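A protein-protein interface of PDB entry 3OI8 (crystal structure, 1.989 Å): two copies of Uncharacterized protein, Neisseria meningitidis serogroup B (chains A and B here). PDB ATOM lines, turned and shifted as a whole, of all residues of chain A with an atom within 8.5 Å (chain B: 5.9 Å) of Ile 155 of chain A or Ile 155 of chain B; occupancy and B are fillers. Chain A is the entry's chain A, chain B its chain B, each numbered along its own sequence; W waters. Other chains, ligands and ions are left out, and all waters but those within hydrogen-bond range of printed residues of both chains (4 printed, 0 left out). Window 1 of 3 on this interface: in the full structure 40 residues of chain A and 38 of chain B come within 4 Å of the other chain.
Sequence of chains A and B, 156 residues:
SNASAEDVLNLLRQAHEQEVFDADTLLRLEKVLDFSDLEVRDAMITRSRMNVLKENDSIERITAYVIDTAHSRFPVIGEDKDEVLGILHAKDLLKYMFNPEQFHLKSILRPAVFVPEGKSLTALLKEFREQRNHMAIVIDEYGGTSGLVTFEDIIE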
ATOM      1  N   ARG A  28      29.487 -11.201  24.979  1.00  0.00           N
ATOM      2  CA  ARG A  28      28.430 -12.201  24.943  1.00  0.00           C
ATOM      3  C   ARG A  28      28.207 -12.765  26.349  1.00  0.00           C
ATOM      4  O   ARG A  28      27.067 -12.943  26.780  1.00  0.00           O
ATOM      5  CB  ARG A  28      28.780 -13.302  23.948  1.00  0.00           C
ATOM      6  CG  ARG A  28      27.596 -14.105  23.458  1.00  0.00           C
ATOM      7  CD  ARG A  28      28.017 -15.142  22.410  1.00  0.00           C
ATOM      8  NE  ARG A  28      27.056 -16.240  22.365  1.00  0.00           N
ATOM      9  CZ  ARG A  28      27.197 -17.346  21.645  1.00  0.00           C
ATOM     10  NH1 ARG A  28      26.256 -18.277  21.700  1.00  0.00           N
ATOM     11  NH2 ARG A  28      28.270 -17.530  20.876  1.00  0.00           N
ATOM     12  N   LYS A  31      26.455 -10.233  28.560  1.00  0.00           N
ATOM     13  CA  LYS A  31      25.046 -10.148  28.175  1.00  0.00           C
ATOM     14  C   LYS A  31      24.249 -11.282  28.829  1.00  0.00           C
ATOM     15  O   LYS A  31      23.161 -11.066  29.352  1.00  0.00           O
ATOM     16  CB  LYS A  31      24.895 -10.183  26.651  1.00  0.00           C
ATOM     17  CG  LYS A  31      23.523  -9.754  26.163  1.00  0.00           C
ATOM     18  CD  LYS A  31      23.412  -9.824  24.642  1.00  0.00           C
ATOM     19  CE  LYS A  31      22.048  -9.331  24.154  1.00  0.00           C
ATOM     20  NZ  LYS A  31      20.913 -10.063  24.795  1.00  0.00           N
ATOM     21  N   VAL A  32      24.814 -12.489  28.819  1.00  0.00           N
ATOM     22  CA  VAL A  32      24.172 -13.635  29.457  1.00  0.00           C
ATOM     23  C   VAL A  32      23.993 -13.385  30.943  1.00  0.00           C
ATOM     24  O   VAL A  32      22.952 -13.689  31.524  1.00  0.00           O
ATOM     25  CB  VAL A  32      24.985 -14.920  29.267  1.00  0.00           C
ATOM     26  CG1 VAL A  32      24.537 -15.976  30.275  1.00  0.00           C
ATOM     27  CG2 VAL A  32      24.836 -15.423  27.836  1.00  0.00           C
ATOM     28  N   PHE A  35      21.233 -10.916  31.446  1.00  0.00           N
ATOM     29  CA  PHE A  35      19.992 -11.584  31.078  1.00  0.00           C
ATOM     30  C   PHE A  35      19.445 -12.415  32.242  1.00  0.00           C
ATOM     31  O   PHE A  35      18.228 -12.527  32.426  1.00  0.00           O
ATOM     32  CB  PHE A  35      20.262 -12.468  29.857  1.00  0.00           C
ATOM     33  CG  PHE A  35      19.041 -13.123  29.273  1.00  0.00           C
ATOM     34  CD1 PHE A  35      18.272 -12.465  28.319  1.00  0.00           C
ATOM     35  CD2 PHE A  35      18.704 -14.424  29.625  1.00  0.00           C
ATOM     36  CE1 PHE A  35      17.158 -13.087  27.750  1.00  0.00           C
ATOM     37  CE2 PHE A  35      17.589 -15.061  29.058  1.00  0.00           C
ATOM     38  CZ  PHE A  35      16.823 -14.395  28.118  1.00  0.00           C
ATOM     39  N   ALA A  43      10.373  -7.843  29.780  1.00  0.00           N
ATOM     40  CA  ALA A  43      10.412  -7.998  28.322  1.00  0.00           C
ATOM     41  C   ALA A  43       9.031  -8.051  27.690  1.00  0.00           C
ATOM     42  O   ALA A  43       8.902  -8.068  26.469  1.00  0.00           O
ATOM     43  CB  ALA A  43      11.209  -9.257  27.919  1.00  0.00           C
ATOM     44  N   LEU A 121      13.592 -14.934  32.666  1.00  0.00           N
ATOM     45  CA  LEU A 121      13.749 -15.015  31.222  1.00  0.00           C
ATOM     46  C   LEU A 121      14.576 -16.220  30.788  1.00  0.00           C
ATOM     47  O   LEU A 121      14.340 -16.775  29.712  1.00  0.00           O
ATOM     48  CB  LEU A 121      14.345 -13.730  30.650  1.00  0.00           C
ATOM     49  CG  LEU A 121      13.478 -12.473  30.643  1.00  0.00           C
ATOM     50  CD1 LEU A 121      14.140 -11.399  29.792  1.00  0.00           C
ATOM     51  CD2 LEU A 121      12.077 -12.772  30.125  1.00  0.00           C
ATOM     52  N   LEU A 125      13.199 -18.733  28.191  1.00  0.00           N
ATOM     53  CA  LEU A 125      13.934 -19.003  26.959  1.00  0.00           C
ATOM     54  C   LEU A 125      14.083 -20.502  26.754  1.00  0.00           C
ATOM     55  O   LEU A 125      13.933 -20.998  25.637  1.00  0.00           O
ATOM     56  CB  LEU A 125      15.296 -18.312  26.961  1.00  0.00           C
ATOM     57  CG  LEU A 125      16.220 -18.724  25.813  1.00  0.00           C
ATOM     58  CD1 LEU A 125      15.532 -18.508  24.461  1.00  0.00           C
ATOM     59  CD2 LEU A 125      17.506 -17.934  25.890  1.00  0.00           C
ATOM     60  N   PHE A 128      10.687 -21.867  25.665  1.00  0.00           N
ATOM     61  CA  PHE A 128      10.418 -21.516  24.269  1.00  0.00           C
ATOM     62  C   PHE A 128      11.186 -22.454  23.341  1.00  0.00           C
ATOM     63  O   PHE A 128      10.640 -22.927  22.344  1.00  0.00           O
ATOM     64  CB  PHE A 128      10.841 -20.087  23.965  1.00  0.00           C
ATOM     65  CG  PHE A 128       9.790 -19.050  24.310  1.00  0.00           C
ATOM     66  CD1 PHE A 128       8.446 -19.352  24.227  1.00  0.00           C
ATOM     67  CD2 PHE A 128      10.161 -17.767  24.669  1.00  0.00           C
ATOM     68  CE1 PHE A 128       7.482 -18.386  24.516  1.00  0.00           C
ATOM     69  CE2 PHE A 128       9.209 -16.797  24.961  1.00  0.00           C
ATOM     70  CZ  PHE A 128       7.868 -17.111  24.886  1.00  0.00           C
ATOM     71  N   ARG A 129      12.455 -22.705  23.660  1.00  0.00           N
ATOM     72  CA  ARG A 129      13.300 -23.522  22.781  1.00  0.00           C
ATOM     73  C   ARG A 129      12.817 -24.969  22.764  1.00  0.00           C
ATOM     74  O   ARG A 129      12.785 -25.606  21.717  1.00  0.00           O
ATOM     75  CB  ARG A 129      14.788 -23.417  23.168  1.00  0.00           C
ATOM     76  CG  ARG A 129      15.475 -22.141  22.653  1.00  0.00           C
ATOM     77  CD  ARG A 129      16.922 -21.996  23.141  1.00  0.00           C
ATOM     78  NE  ARG A 129      17.856 -22.903  22.469  1.00  0.00           N
ATOM     79  CZ  ARG A 129      19.037 -23.271  22.971  1.00  0.00           C
ATOM     80  NH1 ARG A 129      19.432 -22.819  24.158  1.00  0.00           N
ATOM     81  NH2 ARG A 129      19.824 -24.097  22.291  1.00  0.00           N
ATOM     82  N   HIS A 134       6.797 -19.642  20.619  1.00  0.00           N
ATOM     83  CA  HIS A 134       7.292 -18.300  20.296  1.00  0.00           C
ATOM     84  C   HIS A 134       6.646 -17.183  21.117  1.00  0.00           C
ATOM     85  O   HIS A 134       7.191 -16.085  21.229  1.00  0.00           O
ATOM     86  CB  HIS A 134       7.096 -18.006  18.811  1.00  0.00           C
ATOM     87  CG  HIS A 134       8.067 -18.722  17.931  1.00  0.00           C
ATOM     88  ND1 HIS A 134       7.736 -19.860  17.228  1.00  0.00           N
ATOM     89  CD2 HIS A 134       9.372 -18.477  17.664  1.00  0.00           C
ATOM     90  CE1 HIS A 134       8.795 -20.282  16.558  1.00  0.00           C
ATOM     91  NE2 HIS A 134       9.800 -19.460  16.804  1.00  0.00           N
ATOM     92  N   VAL A 149       4.467 -12.093  25.942  1.00  0.00           N
ATOM     93  CA  VAL A 149       5.922 -12.063  25.799  1.00  0.00           C
ATOM     94  C   VAL A 149       6.324 -12.987  24.655  1.00  0.00           C
ATOM     95  O   VAL A 149       5.709 -14.056  24.460  1.00  0.00           O
ATOM     96  CB  VAL A 149       6.660 -12.395  27.147  1.00  0.00           C
ATOM     97  CG1 VAL A 149       6.235 -13.744  27.703  1.00  0.00           C
ATOM     98  CG2 VAL A 149       8.192 -12.307  26.983  1.00  0.00           C
ATOM     99  N   THR A 150       7.313 -12.555  23.870  1.00  0.00           N
ATOM    100  CA  THR A 150       7.724 -13.318  22.698  1.00  0.00           C
ATOM    101  C   THR A 150       9.213 -13.683  22.709  1.00  0.00           C
ATOM    102  O   THR A 150      10.042 -12.978  23.285  1.00  0.00           O
ATOM    103  CB  THR A 150       7.437 -12.539  21.384  1.00  0.00           C
ATOM    104  OG1 THR A 150       8.379 -11.469  21.261  1.00  0.00           O
ATOM    105  CG2 THR A 150       6.012 -11.949  21.387  1.00  0.00           C
ATOM    106  N   PHE A 151       9.509 -14.805  22.060  1.00  0.00           N
ATOM    107  CA  PHE A 151      10.863 -15.306  21.846  1.00  0.00           C
ATOM    108  C   PHE A 151      11.726 -14.233  21.200  1.00  0.00           C
ATOM    109  O   PHE A 151      12.799 -13.895  21.695  1.00  0.00           O
ATOM    110  CB  PHE A 151      10.787 -16.555  20.956  1.00  0.00           C
ATOM    111  CG  PHE A 151      12.132 -17.102  20.531  1.00  0.00           C
ATOM    112  CD1 PHE A 151      12.925 -17.805  21.426  1.00  0.00           C
ATOM    113  CD2 PHE A 151      12.576 -16.945  19.223  1.00  0.00           C
ATOM    114  CE1 PHE A 151      14.163 -18.316  21.034  1.00  0.00           C
ATOM    115  CE2 PHE A 151      13.805 -17.453  18.822  1.00  0.00           C
ATOM    116  CZ  PHE A 151      14.601 -18.141  19.730  1.00  0.00           C
ATOM    117  N   GLU A 152      11.239 -13.662  20.110  1.00  0.00           N
ATOM    118  CA  GLU A 152      12.038 -12.695  19.370  1.00  0.00           C
ATOM    119  C   GLU A 152      12.364 -11.456  20.193  1.00  0.00           C
ATOM    120  O   GLU A 152      13.418 -10.844  20.009  1.00  0.00           O
ATOM    121  CB  GLU A 152      11.378 -12.349  18.032  1.00  0.00           C
ATOM    122  CG  GLU A 152      11.247 -13.572  17.118  1.00  0.00           C
ATOM    123  CD  GLU A 152      10.848 -13.229  15.693  1.00  0.00           C
ATOM    124  OE1 GLU A 152      10.949 -14.121  14.818  1.00  0.00           O
ATOM    125  OE2 GLU A 152      10.439 -12.072  15.445  1.00  0.00           O
ATOM    126  N   ASP A 153      11.481 -11.104  21.124  1.00  0.00           N
ATOM    127  CA  ASP A 153      11.731  -9.974  22.018  1.00  0.00           C
ATOM    128  C   ASP A 153      12.830 -10.260  23.039  1.00  0.00           C
ATOM    129  O   ASP A 153      13.595  -9.371  23.400  1.00  0.00           O
ATOM    130  CB  ASP A 153      10.463  -9.587  22.774  1.00  0.00           C
ATOM    131  CG  ASP A 153       9.580  -8.655  21.988  1.00  0.00           C
ATOM    132  OD1 ASP A 153      10.067  -8.099  20.976  1.00  0.00           O
ATOM    133  OD2 ASP A 153       8.408  -8.475  22.387  1.00  0.00           O
ATOM    134  N   ILE A 154      12.890 -11.489  23.530  1.00  0.00           N
ATOM    135  CA  ILE A 154      13.847 -11.804  24.583  1.00  0.00           C
ATOM    136  C   ILE A 154      15.250 -12.155  24.051  1.00  0.00           C
ATOM    137  O   ILE A 154      16.235 -12.030  24.780  1.00  0.00           O
ATOM    138  CB  ILE A 154      13.318 -12.892  25.558  1.00  0.00           C
ATOM    139  CG1 ILE A 154      13.264 -14.265  24.894  1.00  0.00           C
ATOM    140  CG2 ILE A 154      11.948 -12.511  26.111  1.00  0.00           C
ATOM    141  CD1 ILE A 154      12.830 -15.354  25.865  1.00  0.00           C
ATOM    142  N   ILE A 155      15.337 -12.579  22.790  1.00  0.00           N
ATOM    143  CA  ILE A 155      16.627 -12.933  22.183  1.00  0.00           C
ATOM    144  C   ILE A 155      17.270 -11.721  21.525  1.00  0.00           C
ATOM    145  O   ILE A 155      18.380 -11.809  20.999  1.00  0.00           O
ATOM    146  CB  ILE A 155      16.520 -14.064  21.118  1.00  0.00           C
ATOM    147  CG1 ILE A 155      15.789 -13.571  19.861  1.00  0.00           C
ATOM    148  CG2 ILE A 155      15.887 -15.313  21.701  1.00  0.00           C
ATOM    149  CD1 ILE A 155      15.659 -14.620  18.742  1.00  0.00           C
ATOM    150  N   GLU A 156      16.552 -10.600  21.561  1.00  0.00           N
ATOM    151  CA  GLU A 156      17.026  -9.318  21.059  1.00  0.00           C
ATOM    152  C   GLU A 156      18.456  -9.041  21.516  1.00  0.00           C
ATOM    153  O   GLU A 156      19.210  -8.341  20.837  1.00  0.00           O
ATOM    154  CB  GLU A 156      16.107  -8.197  21.555  1.00  0.00           C
ATOM    155  CG  GLU A 156      15.332  -7.460  20.470  1.00  0.00           C
ATOM    156  CD  GLU A 156      14.416  -6.387  21.040  1.00  0.00           C
ATOM    157  OE1 GLU A 156      14.387  -6.233  22.282  1.00  0.00           O
ATOM    158  OE2 GLU A 156      13.726  -5.700  20.253  1.00  0.00           O
ATOM    159  N   ARG B  28      24.027 -21.678  29.880  1.00  0.00           N
ATOM    160  CA  ARG B  28      24.237 -20.687  28.823  1.00  0.00           C
ATOM    161  C   ARG B  28      25.690 -20.214  28.782  1.00  0.00           C
ATOM    162  O   ARG B  28      26.290 -20.109  27.718  1.00  0.00           O
ATOM    163  CB  ARG B  28      23.316 -19.484  29.018  1.00  0.00           C
ATOM    164  CG  ARG B  28      21.828 -19.837  29.036  1.00  0.00           C
ATOM    165  CD  ARG B  28      20.955 -18.584  28.858  1.00  0.00           C
ATOM    166  NE  ARG B  28      21.030 -18.062  27.499  1.00  0.00           N
ATOM    167  CZ  ARG B  28      21.039 -16.767  27.198  1.00  0.00           C
ATOM    168  NH1 ARG B  28      21.100 -16.370  25.934  1.00  0.00           N
ATOM    169  NH2 ARG B  28      20.980 -15.866  28.166  1.00  0.00           N
ATOM    170  N   LEU B 125      26.113 -14.049  15.144  1.00  0.00           N
ATOM    171  CA  LEU B 125      25.089 -13.689  16.117  1.00  0.00           C
ATOM    172  C   LEU B 125      24.982 -12.177  16.221  1.00  0.00           C
ATOM    173  O   LEU B 125      23.880 -11.604  16.246  1.00  0.00           O
ATOM    174  CB  LEU B 125      25.438 -14.256  17.493  1.00  0.00           C
ATOM    175  CG  LEU B 125      24.455 -15.251  18.111  1.00  0.00           C
ATOM    176  CD1 LEU B 125      24.883 -15.589  19.539  1.00  0.00           C
ATOM    177  CD2 LEU B 125      23.026 -14.704  18.085  1.00  0.00           C
ATOM    178  N   ARG B 129      21.757  -9.711  15.182  1.00  0.00           N
ATOM    179  CA  ARG B 129      21.122  -8.752  16.101  1.00  0.00           C
ATOM    180  C   ARG B 129      21.168  -7.305  15.607  1.00  0.00           C
ATOM    181  O   ARG B 129      20.188  -6.570  15.731  1.00  0.00           O
ATOM    182  CB  ARG B 129      21.713  -8.857  17.506  1.00  0.00           C
ATOM    183  CG  ARG B 129      21.124  -9.987  18.320  1.00  0.00           C
ATOM    184  CD  ARG B 129      21.930 -10.254  19.566  1.00  0.00           C
ATOM    185  NE  ARG B 129      21.288 -11.266  20.390  1.00  0.00           N
ATOM    186  CZ  ARG B 129      21.919 -11.998  21.301  1.00  0.00           C
ATOM    187  NH1 ARG B 129      23.222 -11.832  21.500  1.00  0.00           N
ATOM    188  NH2 ARG B 129      21.246 -12.895  22.014  1.00  0.00           N
ATOM    189  N   HIS B 134      17.480 -12.839  10.342  1.00  0.00           N
ATOM    190  CA  HIS B 134      17.245 -14.138  10.961  1.00  0.00           C
ATOM    191  C   HIS B 134      17.845 -15.307  10.178  1.00  0.00           C
ATOM    192  O   HIS B 134      18.034 -16.376  10.739  1.00  0.00           O
ATOM    193  CB  HIS B 134      15.750 -14.390  11.165  1.00  0.00           C
ATOM    194  CG  HIS B 134      15.206 -13.802  12.430  1.00  0.00           C
ATOM    195  ND1 HIS B 134      14.485 -12.626  12.455  1.00  0.00           N
ATOM    196  CD2 HIS B 134      15.281 -14.225  13.716  1.00  0.00           C
ATOM    197  CE1 HIS B 134      14.142 -12.351  13.701  1.00  0.00           C
ATOM    198  NE2 HIS B 134      14.610 -13.307  14.485  1.00  0.00           N
ATOM    199  N   THR B 150      20.478 -20.041  10.557  1.00  0.00           N
ATOM    200  CA  THR B 150      19.429 -19.216  11.163  1.00  0.00           C
ATOM    201  C   THR B 150      19.790 -18.776  12.580  1.00  0.00           C
ATOM    202  O   THR B 150      20.603 -19.418  13.273  1.00  0.00           O
ATOM    203  CB  THR B 150      18.072 -19.947  11.212  1.00  0.00           C
ATOM    204  OG1 THR B 150      18.193 -21.123  12.028  1.00  0.00           O
ATOM    205  CG2 THR B 150      17.612 -20.348   9.810  1.00  0.00           C
ATOM    206  N   PHE B 151      19.183 -17.672  12.997  1.00  0.00           N
ATOM    207  CA  PHE B 151      19.321 -17.160  14.365  1.00  0.00           C
ATOM    208  C   PHE B 151      18.931 -18.262  15.350  1.00  0.00           C
ATOM    209  O   PHE B 151      19.679 -18.592  16.274  1.00  0.00           O
ATOM    210  CB  PHE B 151      18.406 -15.958  14.535  1.00  0.00           C
ATOM    211  CG  PHE B 151      18.791 -15.045  15.672  1.00  0.00           C
ATOM    212  CD1 PHE B 151      18.694 -13.671  15.530  1.00  0.00           C
ATOM    213  CD2 PHE B 151      19.234 -15.554  16.876  1.00  0.00           C
ATOM    214  CE1 PHE B 151      19.025 -12.818  16.574  1.00  0.00           C
ATOM    215  CE2 PHE B 151      19.572 -14.704  17.923  1.00  0.00           C
ATOM    216  CZ  PHE B 151      19.468 -13.336  17.767  1.00  0.00           C
ATOM    217  N   GLU B 152      17.752 -18.838  15.137  1.00  0.00           N
ATOM    218  CA  GLU B 152      17.265 -19.950  15.954  1.00  0.00           C
ATOM    219  C   GLU B 152      18.331 -21.010  16.257  1.00  0.00           C
ATOM    220  O   GLU B 152      18.430 -21.499  17.386  1.00  0.00           O
ATOM    221  CB  GLU B 152      16.069 -20.612  15.267  1.00  0.00           C
ATOM    222  CG  GLU B 152      14.826 -20.715  16.134  1.00  0.00           C
ATOM    223  CD  GLU B 152      13.540 -20.635  15.322  1.00  0.00           C
ATOM    224  OE1 GLU B 152      13.436 -21.341  14.293  1.00  0.00           O
ATOM    225  OE2 GLU B 152      12.636 -19.862  15.715  1.00  0.00           O
ATOM    226  N   ASP B 153      19.121 -21.372  15.252  1.00  0.00           N
ATOM    227  CA  ASP B 153      20.052 -22.494  15.392  1.00  0.00           C
ATOM    228  C   ASP B 153      21.385 -22.152  16.057  1.00  0.00           C
ATOM    229  O   ASP B 153      22.129 -23.056  16.472  1.00  0.00           O
ATOM    230  CB  ASP B 153      20.321 -23.147  14.027  1.00  0.00           C
ATOM    231  CG  ASP B 153      19.142 -23.968  13.525  1.00  0.00           C
ATOM    232  OD1 ASP B 153      18.133 -24.074  14.253  1.00  0.00           O
ATOM    233  OD2 ASP B 153      19.229 -24.513  12.402  1.00  0.00           O
ATOM    234  N   ILE B 154      21.715 -20.868  16.142  1.00  0.00           N
ATOM    235  CA  ILE B 154      23.016 -20.489  16.696  1.00  0.00           C
ATOM    236  C   ILE B 154      22.922 -19.878  18.101  1.00  0.00           C
ATOM    237  O   ILE B 154      23.935 -19.642  18.755  1.00  0.00           O
ATOM    238  CB  ILE B 154      23.797 -19.535  15.756  1.00  0.00           C
ATOM    239  CG1 ILE B 154      23.128 -18.165  15.710  1.00  0.00           C
ATOM    240  CG2 ILE B 154      23.952 -20.150  14.349  1.00  0.00           C
ATOM    241  CD1 ILE B 154      23.947 -17.124  15.013  1.00  0.00           C
ATOM    242  N   ILE B 155      21.701 -19.633  18.557  1.00  0.00           N
ATOM    243  CA  ILE B 155      21.486 -19.059  19.876  1.00  0.00           C
ATOM    244  C   ILE B 155      21.497 -20.140  20.960  1.00  0.00           C
ATOM    245  O   ILE B 155      22.204 -20.021  21.964  1.00  0.00           O
ATOM    246  CB  ILE B 155      20.159 -18.303  19.931  1.00  0.00           C
ATOM    247  CG1 ILE B 155      20.215 -17.224  21.011  1.00  0.00           C
ATOM    248  CG2 ILE B 155      19.010 -19.275  20.159  1.00  0.00           C
ATOM    249  CD1 ILE B 155      19.065 -16.271  20.955  1.00  0.00           C
HETATM  250  O   HOH W   1      21.221 -16.073  31.174  1.00  0.00           O
HETATM  251  O   HOH W   2      17.968  -7.869  17.668  1.00  0.00           O
HETATM  252  O   HOH W   3      16.533 -22.116  19.542  1.00  0.00           O
HETATM  253  O   HOH W   4      12.137 -17.001  14.896  1.00  0.00           O
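A ring nitrogen (NE2) of His 134 of chain A is in hydrogen-bond range of the side-chain carboxylate of Glu 152 of chain B (3.1 Å).
NE of Arg 129 of chain B sits at hydrogen-bond distance from O of Ile 155 of chain A (3.0 Å).
O of His 134 of chain A lies within hydrogen-bond range of N of Phe 151 of chain A, 2.8 Å away.
The backbone NH of Phe 151 of chain B lies within hydrogen-bond range of the backbone carbonyl oxygen of His 134 of chain B (2.8 Å).
Among the printed residues, pairs that only touch across the chains: Arg 28 of chain A with Leu 125 of chain B, Arg 28 of chain A with Ile 154 of chain B, Lys 31 of chain A with Arg 129 of chain B, Val 32 of chain A with Arg 28 of chain B, Phe 35 of chain A with Arg 28 of chain B, Leu 125 of chain A with Arg 28 of chain B, Glu 152 of chain A with His 134 of chain B, Ile 155 of chain A with Phe 151 of chain B, Ile 155 of chain A with Ile 155 of chain B and Glu 156 of chain A with Arg 129 of chain B.
Printed residues of chain B within 4 Å of Leu 125 of chain A: Arg 28.
Of the printed residues of chain B, His 134 of chain A touches Glu 152 (3.1 Å).
Val 149 of chain A touches none of the printed residues of chain B.
Ile 155 of chain A touches just these residues of chain B: Arg 129 (3.0 Å), Phe 151 (3.7 Å) and Ile 155 (3.4 Å).
Printed residues of chain A within 4 Å of Leu 125 of chain B: Arg 28.
Of the printed residues of chain A, Arg 129 of chain B touches Lys 31, Ile 155 and Glu 156.
Thr 150 of chain B touches none of the printed residues of chain A.
Of chain A, only Ile 155 comes within 4 Å of Ile 155 of chain B.
The nearest residue of chain B that does not touch Ile 155 of chain A is His 134 of chain B (4.6 Å).
The nearest residue of chain A that does not touch Ile 155 of chain B is Arg 28 of chain A (4.4 Å).
The nearest printed residue of chain B that does not touch Glu 152 of chain A is Glu 152 of chain B (6.1 Å).
Of the 10 printed residues of chain B, 8 touch a printed residue of chain A.
Printed residues of chain B that touch a printed residue of chain A: Arg 28, Leu 125, Arg 129, His 134, Phe 151, Glu 152, Ile 154 and Ile 155.
Of the 18 printed residues of chain A, 9 touch a printed residue of chain B.
Among the printed residues, 12 pairs touch across the chains.
Among the printed residues, no Asp or Glu carboxylate lies within 4 Å of a Lys or Arg side-chain nitrogen of the other chain.
Arg 28 of chain A touches Leu 125 of chain B, and with the chains exchanged Leu 125 of chain A touches Arg 28 of chain B.
His 134 of chain A touches Glu 152 of chain B, and with the chains exchanged Glu 152 of chain A touches His 134 of chain B.
Ile 155 of chain A touches Arg 129 of chain B, but with the chains exchanged Arg 129 of chain A does not touch Ile 155 of chain B (4.5 Å).
Ile 155 of chain A touches Phe 151 of chain B, but with the chains exchanged Phe 151 of chain A does not touch Ile 155 of chain B (4.6 Å).
Of the 12 pairs that touch across the chains among the printed residues, 5 have their exchanged pair printed and touching as well.
Water W3 bridges O of Glu 152 of chain B (2.9 Å) and NE of Arg 129 of chain A (3.3 Å).
Water W1 lies within hydrogen-bond range of the backbone carbonyl oxygen (O) of Val 32 of chain A (3.0 Å) and the guanidinium group (NH2) of Arg 28 of chain B (3.0 Å).
Water W4 bridges the side-chain carboxylate (OE2) of Glu 152 of chain B (3.0 Å) and the side-chain carboxylate (OE1) of Glu 152 of chain A (3.1 Å).
Water W2 bridges O of Arg 129 of chain B (3.2 Å) and O of Glu 156 of chain A (3.4 Å).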
